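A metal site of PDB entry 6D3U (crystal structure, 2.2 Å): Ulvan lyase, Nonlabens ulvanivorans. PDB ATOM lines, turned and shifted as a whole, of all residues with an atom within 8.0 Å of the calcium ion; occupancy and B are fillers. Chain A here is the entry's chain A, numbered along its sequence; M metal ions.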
ATOM      1  N   THR A  56      11.443  13.341  24.874  1.00  0.00           N
ATOM      2  CA  THR A  56      11.762  12.717  23.590  1.00  0.00           C
ATOM      3  C   THR A  56      10.449  12.376  22.903  1.00  0.00           C
ATOM      4  O   THR A  56       9.410  12.220  23.558  1.00  0.00           O
ATOM      5  CB  THR A  56      12.597  11.446  23.743  1.00  0.00           C
ATOM      6  OG1 THR A  56      11.762  10.418  24.297  1.00  0.00           O
ATOM      7  CG2 THR A  56      13.794  11.672  24.670  1.00  0.00           C
ATOM      8  N   ASN A  57      10.506  12.283  21.572  1.00  0.00           N
ATOM      9  CA  ASN A  57       9.321  11.928  20.805  1.00  0.00           C
ATOM     10  C   ASN A  57       8.696  10.644  21.351  1.00  0.00           C
ATOM     11  O   ASN A  57       7.508  10.609  21.697  1.00  0.00           O
ATOM     12  CB  ASN A  57       9.658  11.752  19.319  1.00  0.00           C
ATOM     13  CG  ASN A  57       9.916  13.076  18.598  1.00  0.00           C
ATOM     14  OD1 ASN A  57       9.736  14.161  19.149  1.00  0.00           O
ATOM     15  ND2 ASN A  57      10.286  12.974  17.334  1.00  0.00           N
ATOM     16  N   GLN A  58       9.490   9.587  21.430  1.00  0.00           N
ATOM     17  CA  GLN A  58       9.005   8.280  21.819  1.00  0.00           C
ATOM     18  C   GLN A  58       8.432   8.255  23.225  1.00  0.00           C
ATOM     19  O   GLN A  58       7.838   7.244  23.624  1.00  0.00           O
ATOM     20  CB  GLN A  58      10.144   7.252  21.717  1.00  0.00           C
ATOM     21  CG  GLN A  58      11.421   7.629  22.534  1.00  0.00           C
ATOM     22  CD  GLN A  58      12.501   8.417  21.718  1.00  0.00           C
ATOM     23  OE1 GLN A  58      12.172   9.162  20.775  1.00  0.00           O
ATOM     24  NE2 GLN A  58      13.773   8.252  22.102  1.00  0.00           N
ATOM     25  N   GLY A  59       8.616   9.320  24.008  1.00  0.00           N
ATOM     26  CA  GLY A  59       8.065   9.328  25.335  1.00  0.00           C
ATOM     27  C   GLY A  59       7.034  10.415  25.579  1.00  0.00           C
ATOM     28  O   GLY A  59       6.659  10.657  26.724  1.00  0.00           O
ATOM     29  N   THR A  60       6.609  11.109  24.526  1.00  0.00           N
ATOM     30  CA  THR A  60       5.658  12.216  24.686  1.00  0.00           C
ATOM     31  C   THR A  60       4.279  11.643  24.425  1.00  0.00           C
ATOM     32  O   THR A  60       3.723  11.788  23.337  1.00  0.00           O
ATOM     33  CB  THR A  60       6.019  13.400  23.780  1.00  0.00           C
ATOM     34  OG1 THR A  60       7.321  13.865  24.121  1.00  0.00           O
ATOM     35  CG2 THR A  60       5.061  14.565  23.974  1.00  0.00           C
ATOM     36  N   ASN A  61       3.757  10.950  25.439  1.00  0.00           N
ATOM     37  CA  ASN A  61       2.445  10.307  25.341  1.00  0.00           C
ATOM     38  C   ASN A  61       1.335  11.341  25.400  1.00  0.00           C
ATOM     39  O   ASN A  61       1.446  12.337  26.119  1.00  0.00           O
ATOM     40  CB  ASN A  61       2.293   9.275  26.468  1.00  0.00           C
ATOM     41  CG  ASN A  61       2.682   9.822  27.844  1.00  0.00           C
ATOM     42  OD1 ASN A  61       3.863  10.102  28.122  1.00  0.00           O
ATOM     43  ND2 ASN A  61       1.697   9.979  28.712  1.00  0.00           N
ATOM     44  N   PRO A  62       0.236  11.141  24.665  1.00  0.00           N
ATOM     45  CA  PRO A  62      -0.850  12.132  24.688  1.00  0.00           C
ATOM     46  C   PRO A  62      -1.750  12.048  25.917  1.00  0.00           C
ATOM     47  O   PRO A  62      -2.419  13.036  26.244  1.00  0.00           O
ATOM     48  CB  PRO A  62      -1.634  11.827  23.413  1.00  0.00           C
ATOM     49  CG  PRO A  62      -1.399  10.360  23.218  1.00  0.00           C
ATOM     50  CD  PRO A  62      -0.001  10.073  23.681  1.00  0.00           C
ATOM     51  N   THR A  63      -1.790  10.900  26.585  1.00  0.00           N
ATOM     52  CA  THR A  63      -2.648  10.744  27.747  1.00  0.00           C
ATOM     53  C   THR A  63      -1.923   9.907  28.797  1.00  0.00           C
ATOM     54  O   THR A  63      -1.052   9.093  28.469  1.00  0.00           O
ATOM     55  CB  THR A  63      -3.978  10.088  27.401  1.00  0.00           C
ATOM     56  OG1 THR A  63      -3.726   8.789  26.857  1.00  0.00           O
ATOM     57  CG2 THR A  63      -4.732  10.928  26.367  1.00  0.00           C
ATOM     58  N   ARG A  64      -2.308  10.109  30.056  1.00  0.00           N
ATOM     59  CA  ARG A  64      -1.686   9.413  31.165  1.00  0.00           C
ATOM     60  C   ARG A  64      -1.859   7.896  31.034  1.00  0.00           C
ATOM     61  O   ARG A  64      -0.993   7.129  31.482  1.00  0.00           O
ATOM     62  CB  ARG A  64      -2.284   9.936  32.466  1.00  0.00           C
ATOM     63  CG  ARG A  64      -1.835  11.357  32.830  1.00  0.00           C
ATOM     64  CD  ARG A  64      -2.618  11.852  34.065  1.00  0.00           C
ATOM     65  NE  ARG A  64      -2.832  10.778  35.018  1.00  0.00           N
ATOM     66  CZ  ARG A  64      -4.018  10.350  35.457  1.00  0.00           C
ATOM     67  NH1 ARG A  64      -5.153  10.920  35.078  1.00  0.00           N
ATOM     68  NH2 ARG A  64      -4.033   9.369  36.310  1.00  0.00           N
ATOM     69  N   THR A  66      -1.550   5.956  28.443  1.00  0.00           N
ATOM     70  CA  THR A  66      -0.909   5.380  27.259  1.00  0.00           C
ATOM     71  C   THR A  66      -0.069   4.178  27.677  1.00  0.00           C
ATOM     72  O   THR A  66       0.796   4.298  28.546  1.00  0.00           O
ATOM     73  CB  THR A  66      -0.023   6.424  26.577  1.00  0.00           C
ATOM     74  OG1 THR A  66      -0.824   7.491  26.064  1.00  0.00           O
ATOM     75  CG2 THR A  66       0.794   5.778  25.435  1.00  0.00           C
ATOM     76  N   ILE A  77      -1.549   1.846  33.920  1.00  0.00           N
ATOM     77  CA  ILE A  77      -0.444   2.782  33.682  1.00  0.00           C
ATOM     78  C   ILE A  77      -0.874   4.202  34.021  1.00  0.00           C
ATOM     79  O   ILE A  77      -2.032   4.599  33.810  1.00  0.00           O
ATOM     80  CB  ILE A  77       0.035   2.684  32.233  1.00  0.00           C
ATOM     81  CG1 ILE A  77       1.417   3.303  32.123  1.00  0.00           C
ATOM     82  CG2 ILE A  77      -0.946   3.434  31.315  1.00  0.00           C
ATOM     83  CD1 ILE A  77       2.515   2.520  32.845  1.00  0.00           C
ATOM     84  N   ASP A  78       0.042   4.983  34.567  1.00  0.00           N
ATOM     85  CA  ASP A  78      -0.156   6.396  34.900  1.00  0.00           C
ATOM     86  C   ASP A  78       1.149   7.039  34.467  1.00  0.00           C
ATOM     87  O   ASP A  78       2.115   7.069  35.240  1.00  0.00           O
ATOM     88  CB  ASP A  78      -0.447   6.589  36.391  1.00  0.00           C
ATOM     89  CG  ASP A  78      -0.785   8.035  36.766  1.00  0.00           C
ATOM     90  OD1 ASP A  78      -0.767   8.922  35.885  1.00  0.00           O
ATOM     91  OD2 ASP A  78      -1.108   8.266  37.951  1.00  0.00           O
ATOM     92  N   ASP A  79       1.200   7.469  33.200  1.00  0.00           N
ATOM     93  CA  ASP A  79       2.431   7.912  32.565  1.00  0.00           C
ATOM     94  C   ASP A  79       2.448   9.426  32.520  1.00  0.00           C
ATOM     95  O   ASP A  79       1.806  10.035  31.665  1.00  0.00           O
ATOM     96  CB  ASP A  79       2.576   7.305  31.163  1.00  0.00           C
ATOM     97  CG  ASP A  79       3.851   7.798  30.425  1.00  0.00           C
ATOM     98  OD1 ASP A  79       4.478   8.741  30.928  1.00  0.00           O
ATOM     99  OD2 ASP A  79       4.208   7.242  29.369  1.00  0.00           O
ATOM    100  N   ARG A  80       3.174  10.049  33.449  1.00  0.00           N
ATOM    101  CA  ARG A  80       3.361  11.487  33.519  1.00  0.00           C
ATOM    102  C   ARG A  80       4.828  11.832  33.339  1.00  0.00           C
ATOM    103  O   ARG A  80       5.443  12.474  34.208  1.00  0.00           O
ATOM    104  CB  ARG A  80       2.849  12.029  34.854  1.00  0.00           C
ATOM    105  CG  ARG A  80       1.505  11.504  35.272  1.00  0.00           C
ATOM    106  CD  ARG A  80       1.029  12.160  36.560  1.00  0.00           C
ATOM    107  NE  ARG A  80       0.102  11.293  37.290  1.00  0.00           N
ATOM    108  CZ  ARG A  80      -0.513  11.617  38.419  1.00  0.00           C
ATOM    109  NH1 ARG A  80      -0.328  12.825  38.973  1.00  0.00           N
ATOM    110  NH2 ARG A  80      -1.347  10.732  38.994  1.00  0.00           N
ATOM    111  N   SER A  81       5.423  11.399  32.243  1.00  0.00           N
ATOM    112  CA  SER A  81       6.771  11.828  31.884  1.00  0.00           C
ATOM    113  C   SER A  81       6.942  11.772  30.377  1.00  0.00           C
ATOM    114  O   SER A  81       6.676  10.737  29.767  1.00  0.00           O
ATOM    115  CB  SER A  81       7.831  10.945  32.523  1.00  0.00           C
ATOM    116  OG  SER A  81       9.065  11.151  31.838  1.00  0.00           O
ATOM    117  N   CYS A  82       7.411  12.878  29.779  1.00  0.00           N
ATOM    118  CA  CYS A  82       7.620  12.903  28.334  1.00  0.00           C
ATOM    119  C   CYS A  82       9.000  12.383  27.941  1.00  0.00           C
ATOM    120  O   CYS A  82       9.326  12.376  26.751  1.00  0.00           O
ATOM    121  CB  CYS A  82       7.482  14.339  27.778  1.00  0.00           C
ATOM    122  SG  CYS A  82       8.488  15.545  28.705  1.00  0.00           S
ATOM    123  N   TYR A  83       9.777  11.884  28.909  1.00  0.00           N
ATOM    124  CA  TYR A  83      11.073  11.303  28.580  1.00  0.00           C
ATOM    125  C   TYR A  83      10.939   9.934  27.946  1.00  0.00           C
ATOM    126  O   TYR A  83      11.641   9.618  26.967  1.00  0.00           O
ATOM    127  CB  TYR A  83      11.940  11.207  29.834  1.00  0.00           C
ATOM    128  CG  TYR A  83      13.246  10.496  29.539  1.00  0.00           C
ATOM    129  CD1 TYR A  83      14.245  11.122  28.823  1.00  0.00           C
ATOM    130  CD2 TYR A  83      13.471   9.211  29.977  1.00  0.00           C
ATOM    131  CE1 TYR A  83      15.457  10.484  28.544  1.00  0.00           C
ATOM    132  CE2 TYR A  83      14.677   8.560  29.709  1.00  0.00           C
ATOM    133  CZ  TYR A  83      15.664   9.208  28.992  1.00  0.00           C
ATOM    134  OH  TYR A  83      16.859   8.555  28.716  1.00  0.00           O
ATOM    135  N   ALA A  84      10.105   9.063  28.518  1.00  0.00           N
ATOM    136  CA  ALA A  84       9.942   7.709  28.023  1.00  0.00           C
ATOM    137  C   ALA A  84       8.478   7.294  28.144  1.00  0.00           C
ATOM    138  O   ALA A  84       7.670   7.985  28.782  1.00  0.00           O
ATOM    139  CB  ALA A  84      10.862   6.729  28.767  1.00  0.00           C
ATOM    140  N   ASN A  85       8.134   6.184  27.504  1.00  0.00           N
ATOM    141  CA  ASN A  85       6.888   5.479  27.755  1.00  0.00           C
ATOM    142  C   ASN A  85       7.213   4.131  28.380  1.00  0.00           C
ATOM    143  O   ASN A  85       8.368   3.667  28.362  1.00  0.00           O
ATOM    144  CB  ASN A  85       6.059   5.294  26.474  1.00  0.00           C
ATOM    145  CG  ASN A  85       5.390   6.572  26.040  1.00  0.00           C
ATOM    146  OD1 ASN A  85       5.569   7.608  26.637  1.00  0.00           O
ATOM    147  ND2 ASN A  85       4.615   6.501  24.963  1.00  0.00           N
ATOM    148  N   TYR A  86       6.186   3.487  28.928  1.00  0.00           N
ATOM    149  CA  TYR A  86       6.368   2.106  29.366  1.00  0.00           C
ATOM    150  C   TYR A  86       6.758   1.267  28.179  1.00  0.00           C
ATOM    151  O   TYR A  86       6.178   1.399  27.102  1.00  0.00           O
ATOM    152  CB  TYR A  86       5.101   1.543  29.987  1.00  0.00           C
ATOM    153  CG  TYR A  86       5.205   0.061  30.314  1.00  0.00           C
ATOM    154  CD1 TYR A  86       5.696  -0.358  31.548  1.00  0.00           C
ATOM    155  CD2 TYR A  86       4.809  -0.918  29.397  1.00  0.00           C
ATOM    156  CE1 TYR A  86       5.790  -1.699  31.889  1.00  0.00           C
ATOM    157  CE2 TYR A  86       4.898  -2.286  29.715  1.00  0.00           C
ATOM    158  CZ  TYR A  86       5.376  -2.674  30.958  1.00  0.00           C
ATOM    159  OH  TYR A  86       5.475  -3.994  31.298  1.00  0.00           O
ATOM    160  N   ASN A 100      11.572   4.731  33.115  1.00  0.00           N
ATOM    161  CA  ASN A 100      12.624   5.735  33.025  1.00  0.00           C
ATOM    162  C   ASN A 100      12.009   7.126  33.047  1.00  0.00           C
ATOM    163  O   ASN A 100      11.135   7.446  32.232  1.00  0.00           O
ATOM    164  CB  ASN A 100      13.434   5.599  31.737  1.00  0.00           C
ATOM    165  CG  ASN A 100      14.116   4.247  31.594  1.00  0.00           C
ATOM    166  OD1 ASN A 100      14.488   3.589  32.563  1.00  0.00           O
ATOM    167  ND2 ASN A 100      14.300   3.826  30.359  1.00  0.00           N
ATOM    168  N   ILE A 101      12.502   7.981  33.947  1.00  0.00           N
ATOM    169  CA  ILE A 101      12.027   9.357  34.036  1.00  0.00           C
ATOM    170  C   ILE A 101      13.208  10.295  34.242  1.00  0.00           C
ATOM    171  O   ILE A 101      14.246   9.905  34.789  1.00  0.00           O
ATOM    172  CB  ILE A 101      11.008   9.517  35.179  1.00  0.00           C
ATOM    173  CG1 ILE A 101      11.617   9.028  36.500  1.00  0.00           C
ATOM    174  CG2 ILE A 101       9.744   8.773  34.848  1.00  0.00           C
ATOM    175  CD1 ILE A 101      10.755   9.324  37.668  1.00  0.00           C
ATOM    176  N   SER A 105      10.407  16.364  33.348  1.00  0.00           N
ATOM    177  CA  SER A 105       9.785  15.719  32.211  1.00  0.00           C
ATOM    178  C   SER A 105       8.291  15.505  32.395  1.00  0.00           C
ATOM    179  O   SER A 105       7.692  14.722  31.666  1.00  0.00           O
ATOM    180  CB  SER A 105      10.467  14.376  31.915  1.00  0.00           C
ATOM    181  OG  SER A 105      10.265  13.449  32.972  1.00  0.00           O
ATOM    182  N   HIS A 107       4.975  16.449  31.642  1.00  0.00           N
ATOM    183  CA  HIS A 107       4.098  17.180  30.753  1.00  0.00           C
ATOM    184  C   HIS A 107       2.611  16.955  31.044  1.00  0.00           C
ATOM    185  O   HIS A 107       1.762  17.540  30.370  1.00  0.00           O
ATOM    186  CB  HIS A 107       4.385  16.792  29.298  1.00  0.00           C
ATOM    187  CG  HIS A 107       4.076  15.360  28.988  1.00  0.00           C
ATOM    188  ND1 HIS A 107       4.391  14.325  29.842  1.00  0.00           N
ATOM    189  CD2 HIS A 107       3.509  14.786  27.902  1.00  0.00           C
ATOM    190  CE1 HIS A 107       4.019  13.180  29.303  1.00  0.00           C
ATOM    191  NE2 HIS A 107       3.487  13.435  28.123  1.00  0.00           N
ATOM    192  N   MET A 108       2.265  16.175  32.067  1.00  0.00           N
ATOM    193  CA  MET A 108       0.854  15.900  32.349  1.00  0.00           C
ATOM    194  C   MET A 108       0.309  16.700  33.519  1.00  0.00           C
ATOM    195  O   MET A 108      -0.812  17.200  33.466  1.00  0.00           O
ATOM    196  CB  MET A 108       0.670  14.399  32.607  1.00  0.00           C
ATOM    197  CG  MET A 108       0.800  13.548  31.345  1.00  0.00           C
ATOM    198  SD  MET A 108      -0.553  13.837  30.150  1.00  0.00           S
ATOM    199  CE  MET A 108       0.161  13.120  28.684  1.00  0.00           C
ATOM    200  N   ARG A 117       6.452  11.067  36.722  1.00  0.00           N
ATOM    201  CA  ARG A 117       6.345   9.674  37.153  1.00  0.00           C
ATOM    202  C   ARG A 117       5.893   8.806  35.997  1.00  0.00           C
ATOM    203  O   ARG A 117       5.273   9.287  35.059  1.00  0.00           O
ATOM    204  CB  ARG A 117       5.332   9.494  38.295  1.00  0.00           C
ATOM    205  CG  ARG A 117       3.900   9.443  37.788  1.00  0.00           C
ATOM    206  CD  ARG A 117       2.879   9.300  38.904  1.00  0.00           C
ATOM    207  NE  ARG A 117       2.660  10.517  39.688  1.00  0.00           N
ATOM    208  CZ  ARG A 117       2.224  10.515  40.951  1.00  0.00           C
ATOM    209  NH1 ARG A 117       1.994   9.364  41.570  1.00  0.00           N
ATOM    210  NH2 ARG A 117       2.008  11.654  41.615  1.00  0.00           N
ATOM    211  N   ILE A 118       6.232   7.527  36.066  1.00  0.00           N
ATOM    212  CA  ILE A 118       5.549   6.500  35.300  1.00  0.00           C
ATOM    213  C   ILE A 118       5.233   5.377  36.276  1.00  0.00           C
ATOM    214  O   ILE A 118       6.142   4.688  36.740  1.00  0.00           O
ATOM    215  CB  ILE A 118       6.368   5.962  34.125  1.00  0.00           C
ATOM    216  CG1 ILE A 118       6.805   7.100  33.197  1.00  0.00           C
ATOM    217  CG2 ILE A 118       5.507   4.903  33.375  1.00  0.00           C
ATOM    218  CD1 ILE A 118       7.760   6.633  32.057  1.00  0.00           C
HETATM  219 CA    CA M   1       5.728   9.005  28.625  1.00  0.00          CA
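The backbone carbonyl oxygen of Asn 61 sits at hydrogen-bond distance from a ring nitrogen (NE2) of His 107.
The side-chain amide nitrogen (ND2) of Asn 61 sits at hydrogen-bond distance from the backbone carbonyl oxygen (O) of Thr 63.
N of Tyr 83 lies within hydrogen-bond range of OG of Ser 81 (3.1 Å).
The side-chain hydroxyl (OG) of Ser 81 lies within hydrogen-bond range of the side-chain hydroxyl (OG) of Ser 105, 2.8 Å away.
N of Asp 79 is in hydrogen-bond range of O of Arg 64 (2.8 Å).
The side-chain hydroxyl (OG1) of Thr 56 lies within hydrogen-bond range of the backbone NH (N) of Gly 59 (3.3 Å).
Of the 27 residues printed, 6 come within 4 Å of the calcium ion.
The nearest printed residue that does not touch the calcium ion is Cys 82 (4.3 Å).
The calcium ion is bound by the backbone carbonyl oxygen (O) of Ala 84 (2.2 Å), the side-chain amide oxygen (OD1) of Asn 61 (2.2 Å), the backbone carbonyl oxygen (O) of Ser 81 (2.3 Å), the side-chain amide oxygen (OD1) of Asn 85 (2.4 Å), the side-chain carboxylate (OD2) of Asp 79 (2.4 Å), the side-chain carboxylate (OD1) of Asp 79 (2.6 Å) and the backbone carbonyl oxygen (O) of Gly 59 (2.7 Å).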
